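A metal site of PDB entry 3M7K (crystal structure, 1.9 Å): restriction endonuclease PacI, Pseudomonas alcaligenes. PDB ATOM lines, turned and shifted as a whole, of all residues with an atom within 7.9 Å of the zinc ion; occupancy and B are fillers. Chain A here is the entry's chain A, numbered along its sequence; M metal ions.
The side-chain sulfur of Cys 27 lies close to the side-chain amino group of Lys 48 (3.4 Å).
The side-chain sulfur of Cys 4 lies close to the backbone NH of Arg 6 (3.5 Å).
The side-chain sulfur of Cys 7 sits close to the guanidinium group of Arg 9, 3.1 Å away.
N of Cys 4 is in hydrogen-bond range of O of Arg 9 (2.9 Å).
O of Cys 4 lies close to NE2 of Gln 8, 3.5 Å away.
SG of Cys 24 sits close to N of Gly 26 (3.6 Å).
SG of Cys 24 lies close to NH2 of Arg 9 (3.2 Å).
The nearest printed residue that does not touch the zinc ion is Arg 9 (4.2 Å).
The zinc ion is bound by SG of Cys 4, SG of Cys 27, SG of Cys 24 and SG of Cys 7.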
ATOM      1  N   GLN A   3     -32.536  18.333 -19.281  1.00  0.00           N
ATOM      2  CA  GLN A   3     -31.085  18.454 -19.137  1.00  0.00           C
ATOM      3  C   GLN A   3     -30.581  19.797 -19.711  1.00  0.00           C
ATOM      4  O   GLN A   3     -31.014  20.215 -20.791  1.00  0.00           O
ATOM      5  CB  GLN A   3     -30.373  17.275 -19.804  1.00  0.00           C
ATOM      6  CG  GLN A   3     -28.853  17.261 -19.627  1.00  0.00           C
ATOM      7  CD  GLN A   3     -28.205  16.010 -20.223  1.00  0.00           C
ATOM      8  OE1 GLN A   3     -28.262  14.933 -19.651  1.00  0.00           O
ATOM      9  NE2 GLN A   3     -27.578  16.170 -21.387  1.00  0.00           N
ATOM     10  N   CYS A   4     -29.669  20.452 -18.985  1.00  0.00           N
ATOM     11  CA  CYS A   4     -29.041  21.695 -19.486  1.00  0.00           C
ATOM     12  C   CYS A   4     -27.879  21.338 -20.413  1.00  0.00           C
ATOM     13  O   CYS A   4     -26.977  20.608 -19.998  1.00  0.00           O
ATOM     14  CB  CYS A   4     -28.537  22.583 -18.348  1.00  0.00           C
ATOM     15  SG  CYS A   4     -27.568  24.065 -18.877  1.00  0.00           S
ATOM     16  N   PRO A   5     -27.885  21.883 -21.639  1.00  0.00           N
ATOM     17  CA  PRO A   5     -26.866  21.487 -22.630  1.00  0.00           C
ATOM     18  C   PRO A   5     -25.471  22.010 -22.265  1.00  0.00           C
ATOM     19  O   PRO A   5     -24.491  21.556 -22.856  1.00  0.00           O
ATOM     20  CB  PRO A   5     -27.362  22.136 -23.918  1.00  0.00           C
ATOM     21  CG  PRO A   5     -28.150  23.307 -23.458  1.00  0.00           C
ATOM     22  CD  PRO A   5     -28.816  22.882 -22.198  1.00  0.00           C
ATOM     23  N   ARG A   6     -25.385  22.917 -21.309  1.00  0.00           N
ATOM     24  CA  ARG A   6     -24.098  23.498 -20.909  1.00  0.00           C
ATOM     25  C   ARG A   6     -23.448  22.776 -19.707  1.00  0.00           C
ATOM     26  O   ARG A   6     -22.285  22.375 -19.812  1.00  0.00           O
ATOM     27  CB  ARG A   6     -24.240  25.008 -20.664  1.00  0.00           C
ATOM     28  CG  ARG A   6     -22.983  25.656 -20.110  1.00  0.00           C
ATOM     29  CD  ARG A   6     -22.005  26.043 -21.190  1.00  0.00           C
ATOM     30  NE  ARG A   6     -21.988  27.488 -21.410  1.00  0.00           N
ATOM     31  CZ  ARG A   6     -20.887  28.228 -21.401  1.00  0.00           C
ATOM     32  NH1 ARG A   6     -19.700  27.662 -21.224  1.00  0.00           N
ATOM     33  NH2 ARG A   6     -20.972  29.539 -21.599  1.00  0.00           N
ATOM     34  N   CYS A   7     -24.190  22.614 -18.609  1.00  0.00           N
ATOM     35  CA  CYS A   7     -23.670  21.892 -17.436  1.00  0.00           C
ATOM     36  C   CYS A   7     -23.965  20.378 -17.469  1.00  0.00           C
ATOM     37  O   CYS A   7     -23.341  19.627 -16.720  1.00  0.00           O
ATOM     38  CB  CYS A   7     -24.194  22.490 -16.124  1.00  0.00           C
ATOM     39  SG  CYS A   7     -25.985  22.429 -15.941  1.00  0.00           S
ATOM     40  N   GLN A   8     -24.920  19.963 -18.296  1.00  0.00           N
ATOM     41  CA  GLN A   8     -25.364  18.564 -18.398  1.00  0.00           C
ATOM     42  C   GLN A   8     -26.238  18.093 -17.228  1.00  0.00           C
ATOM     43  O   GLN A   8     -26.581  16.903 -17.140  1.00  0.00           O
ATOM     44  CB  GLN A   8     -24.190  17.585 -18.614  1.00  0.00           C
ATOM     45  CG  GLN A   8     -23.251  17.963 -19.755  1.00  0.00           C
ATOM     46  CD  GLN A   8     -23.872  17.736 -21.102  1.00  0.00           C
ATOM     47  OE1 GLN A   8     -23.735  16.657 -21.678  1.00  0.00           O
ATOM     48  NE2 GLN A   8     -24.551  18.744 -21.615  1.00  0.00           N
ATOM     49  N   ARG A   9     -26.625  19.016 -16.345  1.00  0.00           N
ATOM     50  CA  ARG A   9     -27.446  18.639 -15.201  1.00  0.00           C
ATOM     51  C   ARG A   9     -28.886  18.388 -15.595  1.00  0.00           C
ATOM     52  O   ARG A   9     -29.415  19.035 -16.514  1.00  0.00           O
ATOM     53  CB  ARG A   9     -27.387  19.696 -14.094  1.00  0.00           C
ATOM     54  CG  ARG A   9     -26.040  19.800 -13.405  1.00  0.00           C
ATOM     55  CD  ARG A   9     -26.069  20.876 -12.329  1.00  0.00           C
ATOM     56  NE  ARG A   9     -26.498  22.169 -12.873  1.00  0.00           N
ATOM     57  CZ  ARG A   9     -26.977  23.165 -12.131  1.00  0.00           C
ATOM     58  NH1 ARG A   9     -27.089  23.008 -10.819  1.00  0.00           N
ATOM     59  NH2 ARG A   9     -27.353  24.308 -12.706  1.00  0.00           N
ATOM     60  N   LEU A  11     -32.516  18.973 -14.571  1.00  0.00           N
ATOM     61  CA  LEU A  11     -33.112  20.088 -13.796  1.00  0.00           C
ATOM     62  C   LEU A  11     -34.583  20.372 -14.096  1.00  0.00           C
ATOM     63  O   LEU A  11     -35.032  20.210 -15.221  1.00  0.00           O
ATOM     64  CB  LEU A  11     -32.363  21.397 -14.085  1.00  0.00           C
ATOM     65  CG  LEU A  11     -30.846  21.466 -14.002  1.00  0.00           C
ATOM     66  CD1 LEU A  11     -30.371  22.726 -14.691  1.00  0.00           C
ATOM     67  CD2 LEU A  11     -30.382  21.427 -12.562  1.00  0.00           C
ATOM     68  N   GLU A  15     -35.478  26.042 -13.080  1.00  0.00           N
ATOM     69  CA  GLU A  15     -34.042  26.325 -13.183  1.00  0.00           C
ATOM     70  C   GLU A  15     -33.699  26.892 -14.574  1.00  0.00           C
ATOM     71  O   GLU A  15     -32.546  27.229 -14.854  1.00  0.00           O
ATOM     72  CB  GLU A  15     -33.237  25.058 -12.869  1.00  0.00           C
ATOM     73  CG  GLU A  15     -31.873  25.337 -12.248  1.00  0.00           C
ATOM     74  CD  GLU A  15     -31.953  26.053 -10.914  1.00  0.00           C
ATOM     75  OE1 GLU A  15     -31.033  26.826 -10.609  1.00  0.00           O
ATOM     76  OE2 GLU A  15     -32.935  25.852 -10.169  1.00  0.00           O
ATOM     77  N   PHE A  16     -34.716  27.032 -15.424  1.00  0.00           N
ATOM     78  CA  PHE A  16     -34.564  27.619 -16.755  1.00  0.00           C
ATOM     79  C   PHE A  16     -35.297  28.963 -16.927  1.00  0.00           C
ATOM     80  O   PHE A  16     -36.210  29.274 -16.163  1.00  0.00           O
ATOM     81  CB  PHE A  16     -35.026  26.607 -17.825  1.00  0.00           C
ATOM     82  CG  PHE A  16     -34.171  25.369 -17.900  1.00  0.00           C
ATOM     83  CD1 PHE A  16     -34.529  24.212 -17.211  1.00  0.00           C
ATOM     84  CD2 PHE A  16     -32.991  25.369 -18.640  1.00  0.00           C
ATOM     85  CE1 PHE A  16     -33.721  23.063 -17.254  1.00  0.00           C
ATOM     86  CE2 PHE A  16     -32.178  24.234 -18.701  1.00  0.00           C
ATOM     87  CZ  PHE A  16     -32.545  23.076 -18.015  1.00  0.00           C
ATOM     88  N   LYS A  22     -31.223  28.905 -23.842  1.00  0.00           N
ATOM     89  CA  LYS A  22     -31.065  27.450 -23.698  1.00  0.00           C
ATOM     90  C   LYS A  22     -30.247  27.060 -22.451  1.00  0.00           C
ATOM     91  O   LYS A  22     -30.327  25.921 -21.988  1.00  0.00           O
ATOM     92  CB  LYS A  22     -30.415  26.857 -24.948  1.00  0.00           C
ATOM     93  CG  LYS A  22     -31.255  26.970 -26.215  1.00  0.00           C
ATOM     94  CD  LYS A  22     -30.409  26.719 -27.463  1.00  0.00           C
ATOM     95  CE  LYS A  22     -31.251  26.770 -28.731  1.00  0.00           C
ATOM     96  NZ  LYS A  22     -30.442  26.480 -29.958  1.00  0.00           N
ATOM     97  N   MET A  23     -29.460  28.007 -21.934  1.00  0.00           N
ATOM     98  CA  MET A  23     -28.670  27.829 -20.711  1.00  0.00           C
ATOM     99  C   MET A  23     -29.561  27.843 -19.440  1.00  0.00           C
ATOM    100  O   MET A  23     -30.542  28.590 -19.380  1.00  0.00           O
ATOM    101  CB  MET A  23     -27.512  28.876 -20.618  1.00  0.00           C
ATOM    102  CG  MET A  23     -27.874  30.364 -20.911  1.00  0.00           C
ATOM    103  SD  MET A  23     -26.503  31.614 -20.815  1.00  0.00           S
ATOM    104  CE  MET A  23     -25.428  30.916 -22.084  1.00  0.00           C
ATOM    105  N   CYS A  24     -29.235  27.018 -18.450  1.00  0.00           N
ATOM    106  CA  CYS A  24     -29.924  27.107 -17.162  1.00  0.00           C
ATOM    107  C   CYS A  24     -29.489  28.389 -16.399  1.00  0.00           C
ATOM    108  O   CYS A  24     -28.499  29.046 -16.777  1.00  0.00           O
ATOM    109  CB  CYS A  24     -29.687  25.855 -16.325  1.00  0.00           C
ATOM    110  SG  CYS A  24     -28.072  25.745 -15.508  1.00  0.00           S
ATOM    111  N   LYS A  25     -30.211  28.717 -15.339  1.00  0.00           N
ATOM    112  CA  LYS A  25     -29.915  29.941 -14.565  1.00  0.00           C
ATOM    113  C   LYS A  25     -28.502  29.862 -13.952  1.00  0.00           C
ATOM    114  O   LYS A  25     -27.798  30.854 -13.906  1.00  0.00           O
ATOM    115  CB  LYS A  25     -30.969  30.174 -13.467  1.00  0.00           C
ATOM    116  CG  LYS A  25     -32.392  30.536 -13.984  1.00  0.00           C
ATOM    117  CD  LYS A  25     -33.428  30.450 -12.856  1.00  0.00           C
ATOM    118  CE  LYS A  25     -34.782  31.043 -13.245  1.00  0.00           C
ATOM    119  NZ  LYS A  25     -35.740  30.959 -12.096  1.00  0.00           N
ATOM    120  N   GLY A  26     -28.104  28.677 -13.497  1.00  0.00           N
ATOM    121  CA  GLY A  26     -26.773  28.493 -12.893  1.00  0.00           C
ATOM    122  C   GLY A  26     -25.646  28.760 -13.874  1.00  0.00           C
ATOM    123  O   GLY A  26     -24.643  29.434 -13.556  1.00  0.00           O
ATOM    124  N   CYS A  27     -25.815  28.240 -15.091  1.00  0.00           N
ATOM    125  CA  CYS A  27     -24.816  28.432 -16.137  1.00  0.00           C
ATOM    126  C   CYS A  27     -24.730  29.887 -16.579  1.00  0.00           C
ATOM    127  O   CYS A  27     -23.637  30.434 -16.752  1.00  0.00           O
ATOM    128  CB  CYS A  27     -25.096  27.521 -17.333  1.00  0.00           C
ATOM    129  SG  CYS A  27     -24.641  25.760 -17.101  1.00  0.00           S
ATOM    130  N   MET A  28     -25.886  30.522 -16.773  1.00  0.00           N
ATOM    131  CA  MET A  28     -25.930  31.928 -17.177  1.00  0.00           C
ATOM    132  C   MET A  28     -25.377  32.816 -16.053  1.00  0.00           C
ATOM    133  O   MET A  28     -24.608  33.737 -16.323  1.00  0.00           O
ATOM    134  CB  MET A  28     -27.354  32.329 -17.599  1.00  0.00           C
ATOM    135  CG  MET A  28     -27.571  33.799 -17.949  1.00  0.00           C
ATOM    136  SD  MET A  28     -27.209  34.276 -19.645  1.00  0.00           S
ATOM    137  CE  MET A  28     -25.410  34.394 -19.628  1.00  0.00           C
ATOM    138  N   LYS A  48     -16.577  26.706 -11.503  1.00  0.00           N
ATOM    139  CA  LYS A  48     -17.965  26.493 -11.956  1.00  0.00           C
ATOM    140  C   LYS A  48     -18.676  25.471 -11.061  1.00  0.00           C
ATOM    141  O   LYS A  48     -19.792  25.716 -10.630  1.00  0.00           O
ATOM    142  CB  LYS A  48     -18.040  26.084 -13.432  1.00  0.00           C
ATOM    143  CG  LYS A  48     -19.482  25.928 -13.928  1.00  0.00           C
ATOM    144  CD  LYS A  48     -19.580  25.881 -15.460  1.00  0.00           C
ATOM    145  CE  LYS A  48     -21.022  26.077 -15.908  1.00  0.00           C
ATOM    146  NZ  LYS A  48     -21.247  25.699 -17.349  1.00  0.00           N
ATOM    147  N   LEU A  52     -21.912  26.202  -8.774  1.00  0.00           N
ATOM    148  CA  LEU A  52     -23.203  25.537  -9.006  1.00  0.00           C
ATOM    149  C   LEU A  52     -23.746  24.898  -7.741  1.00  0.00           C
ATOM    150  O   LEU A  52     -24.951  24.965  -7.488  1.00  0.00           O
ATOM    151  CB  LEU A  52     -23.148  24.528 -10.168  1.00  0.00           C
ATOM    152  CG  LEU A  52     -22.942  25.036 -11.603  1.00  0.00           C
ATOM    153  CD1 LEU A  52     -22.970  23.842 -12.560  1.00  0.00           C
ATOM    154  CD2 LEU A  52     -23.973  26.052 -12.033  1.00  0.00           C
HETATM  155 ZN    ZN M   1     -26.614  24.607 -16.879  1.00  0.00          ZN
